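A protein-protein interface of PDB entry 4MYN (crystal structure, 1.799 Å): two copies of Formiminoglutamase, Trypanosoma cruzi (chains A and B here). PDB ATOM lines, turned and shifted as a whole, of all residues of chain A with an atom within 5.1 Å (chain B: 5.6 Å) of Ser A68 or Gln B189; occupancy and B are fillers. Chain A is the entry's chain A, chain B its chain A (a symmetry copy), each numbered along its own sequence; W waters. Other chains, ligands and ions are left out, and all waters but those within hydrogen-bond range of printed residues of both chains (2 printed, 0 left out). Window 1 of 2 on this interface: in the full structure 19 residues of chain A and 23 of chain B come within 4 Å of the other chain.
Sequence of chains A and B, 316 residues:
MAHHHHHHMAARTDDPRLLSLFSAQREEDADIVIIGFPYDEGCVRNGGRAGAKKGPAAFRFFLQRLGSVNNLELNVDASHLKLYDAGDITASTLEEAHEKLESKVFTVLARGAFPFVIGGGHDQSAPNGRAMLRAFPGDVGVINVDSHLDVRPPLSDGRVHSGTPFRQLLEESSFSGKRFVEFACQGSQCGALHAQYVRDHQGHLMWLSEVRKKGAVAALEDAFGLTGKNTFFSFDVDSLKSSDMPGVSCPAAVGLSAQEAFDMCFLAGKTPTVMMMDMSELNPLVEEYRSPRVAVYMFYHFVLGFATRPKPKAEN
NH1 of Arg B152 lies within salt-bridge range of OD2 of Asp A15, 3.0 Å away. The side-chain carboxylate (OD1) of Asp A15 sits close to the backbone NH (N) of Gly B191 (3.5 Å). NH2 of Arg A17 is in hydrogen-bond range of O of Gln B189, 3.3 Å away. The backbone carbonyl oxygen of Ser B188 lies within hydrogen-bond range of the backbone NH of Ser A68 (3.2 Å). N of Cys B190 sits at hydrogen-bond distance from OG of Ser A68 (3.4 Å). The backbone NH of Ser B188 lies close to the side-chain amide nitrogen of Asn A71 (3.4 Å).
The side-chain carboxylate (OD2) of Asp A15 is in salt-bridge range of the guanidinium group (NH2) of Arg A17 (3.9 Å). OH of Tyr A300 is in hydrogen-bond range of O of Ser A68, 2.6 Å away. The side-chain sulfur (SG) of Cys B190 is in hydrogen-bond range of the backbone carbonyl oxygen (O) of Ser B147 (3.3 Å). A ring nitrogen (NE2) of His B148 is in hydrogen-bond range of the side-chain amide oxygen of Gln B189 (2.9 Å). The side-chain sulfur (SG) of Cys B250 lies within hydrogen-bond range of a ring nitrogen (NE2) of His B148. O of Gln B186 sits at hydrogen-bond distance from SG of Cys B190 (3.3 Å).
Arg B152 touches Arg A17. CA of Gly A67 touches O of Ser B188 (3.6 Å). Ser A68 touches Gly B187. OG of Ser A68 touches N of Gln B189 (3.7 Å). C of Gly B187 touches ND2 of Asn A71, at 3.4 Å. NH2 of Arg A293 touches SG of Cys B250, 3.8 Å away. Arg A293 touches Pro B251. CE1 of Tyr A297 touches CB of Ser B188, at 3.9 Å. OH of Tyr A297 touches CG of Gln B189 (3.8 Å). Ser B188 touches Tyr A300 (CB to CE2, 3.4 Å).
Of the printed residues of chain B, Asp A15 touches Arg B152 and Gly B191. Leu A66 touches none of the printed residues of chain B. Of the printed residues of chain B, Ser A68 touches Gly B187, Ser B188, Gln B189 and Cys B190. Of the printed residues of chain B, Tyr A297 touches Ser B188 and Gln B189. Ser B147 touches none of the printed residues of chain A. Gln B189 touches just these residues of chain A: Arg A17, Ser A68 and Tyr A297. Of the printed residues of chain A, Cys B190 touches Ser A68. Printed residues of chain A within 4 Å of Gly B191: Asp A15. Of the printed residues of chain A, Pro B251 touches Arg A293. The nearest residue of chain A that does not touch Gln B189 is Arg A293 (4.6 Å). The nearest printed residue of chain A that does not touch Cys B250 is Tyr A297 (6.3 Å).
Of the 15 printed residues of chain B, 8 touch a printed residue of chain A.
No position is printed for both chains. Of the 16 pairs that touch across the chains among the printed residues, none has its exchanged pair printed and touching as well.
Water W2 bridges N of Gly B191 (2.8 Å) and OD2 of Asp A15 (3.2 Å). Water W1 lies within hydrogen-bond range of O of Ser B188 (2.8 Å), N of Gly A67 (2.9 Å) and OH of Tyr A297 (2.9 Å).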
ATOM      1  N   ASP A  15     -19.705 -21.978 -22.643  1.00  0.00           N
ATOM      2  CA  ASP A  15     -20.884 -22.205 -21.811  1.00  0.00           C
ATOM      3  C   ASP A  15     -22.168 -22.096 -22.656  1.00  0.00           C
ATOM      4  O   ASP A  15     -22.920 -21.125 -22.545  1.00  0.00           O
ATOM      5  CB  ASP A  15     -20.899 -21.184 -20.668  1.00  0.00           C
ATOM      6  CG  ASP A  15     -21.719 -21.646 -19.469  1.00  0.00           C
ATOM      7  OD1 ASP A  15     -22.398 -22.694 -19.569  1.00  0.00           O
ATOM      8  OD2 ASP A  15     -21.676 -20.948 -18.428  1.00  0.00           O
ATOM      9  N   PRO A  16     -22.419 -23.100 -23.507  1.00  0.00           N
ATOM     10  CA  PRO A  16     -23.527 -23.065 -24.465  1.00  0.00           C
ATOM     11  C   PRO A  16     -24.879 -23.190 -23.776  1.00  0.00           C
ATOM     12  O   PRO A  16     -25.042 -24.066 -22.924  1.00  0.00           O
ATOM     13  CB  PRO A  16     -23.282 -24.306 -25.334  1.00  0.00           C
ATOM     14  CG  PRO A  16     -21.871 -24.732 -25.039  1.00  0.00           C
ATOM     15  CD  PRO A  16     -21.629 -24.335 -23.629  1.00  0.00           C
ATOM     16  N   ARG A  17     -25.831 -22.346 -24.173  1.00  0.00           N
ATOM     17  CA  ARG A  17     -27.151 -22.289 -23.546  1.00  0.00           C
ATOM     18  C   ARG A  17     -28.251 -22.347 -24.611  1.00  0.00           C
ATOM     19  O   ARG A  17     -27.956 -22.581 -25.782  1.00  0.00           O
ATOM     20  CB  ARG A  17     -27.251 -21.031 -22.674  1.00  0.00           C
ATOM     21  CG  ARG A  17     -26.306 -21.075 -21.465  1.00  0.00           C
ATOM     22  CD  ARG A  17     -26.394 -19.846 -20.536  1.00  0.00           C
ATOM     23  NE  ARG A  17     -25.768 -20.124 -19.239  1.00  0.00           N
ATOM     24  CZ  ARG A  17     -25.680 -19.267 -18.221  1.00  0.00           C
ATOM     25  NH1 ARG A  17     -26.176 -18.037 -18.315  1.00  0.00           N
ATOM     26  NH2 ARG A  17     -25.097 -19.645 -17.090  1.00  0.00           N
ATOM     27  N   LEU A  66     -30.282 -17.609 -21.005  1.00  0.00           N
ATOM     28  CA  LEU A  66     -30.359 -18.614 -19.951  1.00  0.00           C
ATOM     29  C   LEU A  66     -30.318 -20.061 -20.433  1.00  0.00           C
ATOM     30  O   LEU A  66     -30.600 -20.347 -21.593  1.00  0.00           O
ATOM     31  CB  LEU A  66     -31.656 -18.408 -19.162  1.00  0.00           C
ATOM     32  CG  LEU A  66     -31.868 -17.054 -18.475  1.00  0.00           C
ATOM     33  CD1 LEU A  66     -33.241 -17.015 -17.782  1.00  0.00           C
ATOM     34  CD2 LEU A  66     -30.746 -16.789 -17.486  1.00  0.00           C
ATOM     35  N   GLY A  67     -29.982 -20.967 -19.516  1.00  0.00           N
ATOM     36  CA  GLY A  67     -30.230 -22.392 -19.689  1.00  0.00           C
ATOM     37  C   GLY A  67     -29.137 -23.239 -20.324  1.00  0.00           C
ATOM     38  O   GLY A  67     -29.138 -23.405 -21.542  1.00  0.00           O
ATOM     39  N   SER A  68     -28.252 -23.809 -19.502  1.00  0.00           N
ATOM     40  CA  SER A  68     -27.146 -24.654 -19.990  1.00  0.00           C
ATOM     41  C   SER A  68     -27.670 -25.849 -20.795  1.00  0.00           C
ATOM     42  O   SER A  68     -28.455 -26.636 -20.284  1.00  0.00           O
ATOM     43  CB  SER A  68     -26.305 -25.163 -18.815  1.00  0.00           C
ATOM     44  OG  SER A  68     -26.015 -24.132 -17.893  1.00  0.00           O
ATOM     45  N   VAL A  69     -27.250 -25.985 -22.053  1.00  0.00           N
ATOM     46  CA  VAL A  69     -27.792 -27.045 -22.909  1.00  0.00           C
ATOM     47  C   VAL A  69     -27.458 -28.440 -22.388  1.00  0.00           C
ATOM     48  O   VAL A  69     -28.236 -29.379 -22.550  1.00  0.00           O
ATOM     49  CB  VAL A  69     -27.329 -26.917 -24.386  1.00  0.00           C
ATOM     50  CG1 VAL A  69     -28.081 -25.794 -25.083  1.00  0.00           C
ATOM     51  CG2 VAL A  69     -25.847 -26.689 -24.448  1.00  0.00           C
ATOM     52  N   ASN A  70     -26.303 -28.566 -21.757  1.00  0.00           N
ATOM     53  CA  ASN A  70     -25.944 -29.812 -21.114  1.00  0.00           C
ATOM     54  C   ASN A  70     -25.964 -29.615 -19.602  1.00  0.00           C
ATOM     55  O   ASN A  70     -25.082 -28.966 -19.032  1.00  0.00           O
ATOM     56  CB  ASN A  70     -24.573 -30.289 -21.589  1.00  0.00           C
ATOM     57  CG  ASN A  70     -24.250 -31.681 -21.103  1.00  0.00           C
ATOM     58  OD1 ASN A  70     -25.049 -32.318 -20.408  1.00  0.00           O
ATOM     59  ND2 ASN A  70     -23.074 -32.164 -21.465  1.00  0.00           N
ATOM     60  N   ASN A  71     -26.994 -30.163 -18.970  1.00  0.00           N
ATOM     61  CA  ASN A  71     -27.257 -29.939 -17.558  1.00  0.00           C
ATOM     62  C   ASN A  71     -26.744 -31.135 -16.757  1.00  0.00           C
ATOM     63  O   ASN A  71     -27.332 -32.229 -16.796  1.00  0.00           O
ATOM     64  CB  ASN A  71     -28.773 -29.764 -17.359  1.00  0.00           C
ATOM     65  CG  ASN A  71     -29.159 -29.526 -15.903  1.00  0.00           C
ATOM     66  OD1 ASN A  71     -28.641 -30.179 -14.993  1.00  0.00           O
ATOM     67  ND2 ASN A  71     -30.093 -28.598 -15.681  1.00  0.00           N
ATOM     68  N   ARG A 293     -37.670 -14.597 -16.161  1.00  0.00           N
ATOM     69  CA  ARG A 293     -36.633 -15.608 -15.947  1.00  0.00           C
ATOM     70  C   ARG A 293     -37.239 -16.962 -15.566  1.00  0.00           C
ATOM     71  O   ARG A 293     -36.839 -18.016 -16.097  1.00  0.00           O
ATOM     72  CB  ARG A 293     -35.618 -15.132 -14.897  1.00  0.00           C
ATOM     73  CG  ARG A 293     -34.711 -13.989 -15.382  1.00  0.00           C
ATOM     74  CD  ARG A 293     -33.805 -13.464 -14.248  1.00  0.00           C
ATOM     75  NE  ARG A 293     -32.776 -14.435 -13.899  1.00  0.00           N
ATOM     76  CZ  ARG A 293     -31.528 -14.413 -14.358  1.00  0.00           C
ATOM     77  NH1 ARG A 293     -31.129 -13.445 -15.176  1.00  0.00           N
ATOM     78  NH2 ARG A 293     -30.669 -15.353 -13.982  1.00  0.00           N
ATOM     79  N   TYR A 297     -36.965 -20.370 -17.660  1.00  0.00           N
ATOM     80  CA  TYR A 297     -36.521 -21.612 -17.000  1.00  0.00           C
ATOM     81  C   TYR A 297     -37.553 -22.748 -17.097  1.00  0.00           C
ATOM     82  O   TYR A 297     -37.194 -23.926 -17.181  1.00  0.00           O
ATOM     83  CB  TYR A 297     -36.111 -21.380 -15.532  1.00  0.00           C
ATOM     84  CG  TYR A 297     -34.707 -20.805 -15.393  1.00  0.00           C
ATOM     85  CD1 TYR A 297     -33.624 -21.415 -16.020  1.00  0.00           C
ATOM     86  CD2 TYR A 297     -34.475 -19.652 -14.662  1.00  0.00           C
ATOM     87  CE1 TYR A 297     -32.346 -20.892 -15.919  1.00  0.00           C
ATOM     88  CE2 TYR A 297     -33.194 -19.122 -14.551  1.00  0.00           C
ATOM     89  CZ  TYR A 297     -32.141 -19.745 -15.183  1.00  0.00           C
ATOM     90  OH  TYR A 297     -30.874 -19.218 -15.065  1.00  0.00           O
ATOM     91  N   TYR A 300     -37.126 -23.995 -20.513  1.00  0.00           N
ATOM     92  CA  TYR A 300     -35.845 -24.698 -20.464  1.00  0.00           C
ATOM     93  C   TYR A 300     -36.005 -26.135 -19.947  1.00  0.00           C
ATOM     94  O   TYR A 300     -35.515 -27.090 -20.555  1.00  0.00           O
ATOM     95  CB  TYR A 300     -34.881 -23.913 -19.578  1.00  0.00           C
ATOM     96  CG  TYR A 300     -33.606 -24.647 -19.235  1.00  0.00           C
ATOM     97  CD1 TYR A 300     -32.639 -24.885 -20.201  1.00  0.00           C
ATOM     98  CD2 TYR A 300     -33.369 -25.088 -17.948  1.00  0.00           C
ATOM     99  CE1 TYR A 300     -31.467 -25.552 -19.892  1.00  0.00           C
ATOM    100  CE2 TYR A 300     -32.204 -25.750 -17.624  1.00  0.00           C
ATOM    101  CZ  TYR A 300     -31.252 -25.979 -18.606  1.00  0.00           C
ATOM    102  OH  TYR A 300     -30.090 -26.636 -18.278  1.00  0.00           O
ATOM    103  N   LEU A 304     -35.312 -29.723 -21.883  1.00  0.00           N
ATOM    104  CA  LEU A 304     -34.517 -30.827 -21.346  1.00  0.00           C
ATOM    105  C   LEU A 304     -35.313 -32.147 -21.347  1.00  0.00           C
ATOM    106  O   LEU A 304     -34.793 -33.193 -21.751  1.00  0.00           O
ATOM    107  CB  LEU A 304     -33.983 -30.502 -19.937  1.00  0.00           C
ATOM    108  CG  LEU A 304     -32.969 -29.363 -19.754  1.00  0.00           C
ATOM    109  CD1 LEU A 304     -32.528 -29.255 -18.289  1.00  0.00           C
ATOM    110  CD2 LEU A 304     -31.764 -29.583 -20.632  1.00  0.00           C
ATOM    111  N   SER B 147     -24.916 -20.617  -6.404  1.00  0.00           N
ATOM    112  CA  SER B 147     -25.636 -21.239  -7.519  1.00  0.00           C
ATOM    113  C   SER B 147     -24.712 -21.471  -8.722  1.00  0.00           C
ATOM    114  O   SER B 147     -24.993 -22.319  -9.572  1.00  0.00           O
ATOM    115  CB  SER B 147     -26.853 -20.403  -7.926  1.00  0.00           C
ATOM    116  OG  SER B 147     -26.481 -19.066  -8.185  1.00  0.00           O
ATOM    117  N   HIS B 148     -23.614 -20.718  -8.783  1.00  0.00           N
ATOM    118  CA  HIS B 148     -22.662 -20.793  -9.905  1.00  0.00           C
ATOM    119  C   HIS B 148     -21.323 -21.402  -9.487  1.00  0.00           C
ATOM    120  O   HIS B 148     -20.984 -21.367  -8.329  1.00  0.00           O
ATOM    121  CB  HIS B 148     -22.415 -19.390 -10.453  1.00  0.00           C
ATOM    122  CG  HIS B 148     -23.662 -18.571 -10.571  1.00  0.00           C
ATOM    123  ND1 HIS B 148     -24.045 -17.653  -9.614  1.00  0.00           N
ATOM    124  CD2 HIS B 148     -24.626 -18.551 -11.525  1.00  0.00           C
ATOM    125  CE1 HIS B 148     -25.189 -17.097  -9.979  1.00  0.00           C
ATOM    126  NE2 HIS B 148     -25.565 -17.628 -11.131  1.00  0.00           N
ATOM    127  N   ARG B 152     -14.889 -19.586 -14.118  1.00  0.00           N
ATOM    128  CA  ARG B 152     -14.792 -18.966 -15.432  1.00  0.00           C
ATOM    129  C   ARG B 152     -13.370 -18.511 -15.717  1.00  0.00           C
ATOM    130  O   ARG B 152     -12.650 -18.079 -14.812  1.00  0.00           O
ATOM    131  CB  ARG B 152     -15.732 -17.763 -15.535  1.00  0.00           C
ATOM    132  CG  ARG B 152     -17.182 -18.086 -15.234  1.00  0.00           C
ATOM    133  CD  ARG B 152     -18.112 -17.180 -16.032  1.00  0.00           C
ATOM    134  NE  ARG B 152     -19.511 -17.554 -15.844  1.00  0.00           N
ATOM    135  CZ  ARG B 152     -20.204 -18.311 -16.691  1.00  0.00           C
ATOM    136  NH1 ARG B 152     -19.638 -18.780 -17.799  1.00  0.00           N
ATOM    137  NH2 ARG B 152     -21.474 -18.596 -16.430  1.00  0.00           N
ATOM    138  N   GLN B 186     -26.269 -24.948  -9.359  1.00  0.00           N
ATOM    139  CA  GLN B 186     -27.465 -25.262 -10.127  1.00  0.00           C
ATOM    140  C   GLN B 186     -27.155 -25.639 -11.570  1.00  0.00           C
ATOM    141  O   GLN B 186     -26.552 -24.855 -12.302  1.00  0.00           O
ATOM    142  CB  GLN B 186     -28.447 -24.089 -10.071  1.00  0.00           C
ATOM    143  CG  GLN B 186     -29.040 -23.845  -8.664  1.00  0.00           C
ATOM    144  CD  GLN B 186     -29.951 -22.631  -8.645  1.00  0.00           C
ATOM    145  OE1 GLN B 186     -30.535 -22.276  -9.666  1.00  0.00           O
ATOM    146  NE2 GLN B 186     -30.074 -21.986  -7.491  1.00  0.00           N
ATOM    147  N   GLY B 187     -27.572 -26.841 -11.963  1.00  0.00           N
ATOM    148  CA  GLY B 187     -27.284 -27.361 -13.291  1.00  0.00           C
ATOM    149  C   GLY B 187     -27.773 -26.490 -14.434  1.00  0.00           C
ATOM    150  O   GLY B 187     -27.181 -26.495 -15.509  1.00  0.00           O
ATOM    151  N   SER B 188     -28.851 -25.742 -14.211  1.00  0.00           N
ATOM    152  CA  SER B 188     -29.378 -24.845 -15.240  1.00  0.00           C
ATOM    153  C   SER B 188     -28.474 -23.638 -15.482  1.00  0.00           C
ATOM    154  O   SER B 188     -28.654 -22.913 -16.457  1.00  0.00           O
ATOM    155  CB  SER B 188     -30.757 -24.338 -14.830  1.00  0.00           C
ATOM    156  OG  SER B 188     -30.667 -23.682 -13.581  1.00  0.00           O
ATOM    157  N   GLN B 189     -27.512 -23.427 -14.584  1.00  0.00           N
ATOM    158  CA  GLN B 189     -26.677 -22.228 -14.592  1.00  0.00           C
ATOM    159  C   GLN B 189     -25.194 -22.574 -14.635  1.00  0.00           C
ATOM    160  O   GLN B 189     -24.352 -21.677 -14.576  1.00  0.00           O
ATOM    161  CB  GLN B 189     -26.882 -21.403 -13.312  1.00  0.00           C
ATOM    162  CG  GLN B 189     -28.305 -21.020 -12.959  1.00  0.00           C
ATOM    163  CD  GLN B 189     -28.349 -19.740 -12.145  1.00  0.00           C
ATOM    164  OE1 GLN B 189     -27.881 -18.688 -12.603  1.00  0.00           O
ATOM    165  NE2 GLN B 189     -28.901 -19.818 -10.931  1.00  0.00           N
ATOM    166  N   CYS B 190     -24.876 -23.865 -14.684  1.00  0.00           N
ATOM    167  CA  CYS B 190     -23.474 -24.291 -14.660  1.00  0.00           C
ATOM    168  C   CYS B 190     -23.110 -25.098 -15.917  1.00  0.00           C
ATOM    169  O   CYS B 190     -23.712 -26.130 -16.203  1.00  0.00           O
ATOM    170  CB  CYS B 190     -23.167 -25.082 -13.372  1.00  0.00           C
ATOM    171  SG  CYS B 190     -23.386 -24.135 -11.795  1.00  0.00           S
ATOM    172  N   GLY B 191     -22.123 -24.618 -16.665  1.00  0.00           N
ATOM    173  CA  GLY B 191     -21.726 -25.268 -17.902  1.00  0.00           C
ATOM    174  C   GLY B 191     -20.939 -26.551 -17.697  1.00  0.00           C
ATOM    175  O   GLY B 191     -20.189 -26.680 -16.726  1.00  0.00           O
ATOM    176  N   ASP B 238     -26.370 -15.218  -3.807  1.00  0.00           N
ATOM    177  CA  ASP B 238     -27.211 -15.598  -4.945  1.00  0.00           C
ATOM    178  C   ASP B 238     -27.459 -17.113  -5.030  1.00  0.00           C
ATOM    179  O   ASP B 238     -28.068 -17.589  -5.988  1.00  0.00           O
ATOM    180  CB  ASP B 238     -26.705 -15.007  -6.278  1.00  0.00           C
ATOM    181  CG  ASP B 238     -25.457 -15.697  -6.825  1.00  0.00           C
ATOM    182  OD1 ASP B 238     -25.180 -16.877  -6.500  1.00  0.00           O
ATOM    183  OD2 ASP B 238     -24.757 -15.039  -7.629  1.00  0.00           O
ATOM    184  N   CYS B 250     -27.283 -11.508  -9.614  1.00  0.00           N
ATOM    185  CA  CYS B 250     -27.869 -12.598 -10.403  1.00  0.00           C
ATOM    186  C   CYS B 250     -28.909 -13.331  -9.562  1.00  0.00           C
ATOM    187  O   CYS B 250     -28.609 -14.366  -8.983  1.00  0.00           O
ATOM    188  CB  CYS B 250     -26.798 -13.602 -10.876  1.00  0.00           C
ATOM    189  SG  CYS B 250     -27.394 -14.921 -12.040  1.00  0.00           S
ATOM    190  N   PRO B 251     -30.132 -12.784  -9.491  1.00  0.00           N
ATOM    191  CA  PRO B 251     -31.194 -13.364  -8.652  1.00  0.00           C
ATOM    192  C   PRO B 251     -31.550 -14.779  -9.072  1.00  0.00           C
ATOM    193  O   PRO B 251     -31.696 -15.064 -10.263  1.00  0.00           O
ATOM    194  CB  PRO B 251     -32.379 -12.417  -8.876  1.00  0.00           C
ATOM    195  CG  PRO B 251     -31.728 -11.108  -9.237  1.00  0.00           C
ATOM    196  CD  PRO B 251     -30.548 -11.506 -10.094  1.00  0.00           C
ATOM    197  N   ALA B 252     -31.688 -15.664  -8.089  1.00  0.00           N
ATOM    198  CA  ALA B 252     -31.925 -17.071  -8.368  1.00  0.00           C
ATOM    199  C   ALA B 252     -33.429 -17.339  -8.399  1.00  0.00           C
ATOM    200  O   ALA B 252     -34.156 -16.814  -7.569  1.00  0.00           O
ATOM    201  CB  ALA B 252     -31.272 -17.925  -7.300  1.00  0.00           C
ATOM    202  N   ALA B 253     -33.900 -18.144  -9.345  1.00  0.00           N
ATOM    203  CA  ALA B 253     -35.325 -18.523  -9.371  1.00  0.00           C
ATOM    204  C   ALA B 253     -35.626 -19.522  -8.260  1.00  0.00           C
ATOM    205  O   ALA B 253     -36.585 -19.359  -7.480  1.00  0.00           O
ATOM    206  CB  ALA B 253     -35.701 -19.122 -10.734  1.00  0.00           C
ATOM    207  N   VAL B 254     -34.801 -20.565  -8.214  1.00  0.00           N
ATOM    208  CA  VAL B 254     -34.814 -21.544  -7.149  1.00  0.00           C
ATOM    209  C   VAL B 254     -33.493 -21.405  -6.387  1.00  0.00           C
ATOM    210  O   VAL B 254     -32.548 -20.752  -6.861  1.00  0.00           O
ATOM    211  CB  VAL B 254     -34.962 -22.983  -7.682  1.00  0.00           C
ATOM    212  CG1 VAL B 254     -36.359 -23.218  -8.328  1.00  0.00           C
ATOM    213  CG2 VAL B 254     -33.878 -23.285  -8.707  1.00  0.00           C
HETATM  214  O   HOH W   1     -28.884 -20.131 -16.984  1.00  0.00           O
HETATM  215  O   HOH W   2     -20.771 -22.381 -15.741  1.00  0.00           O
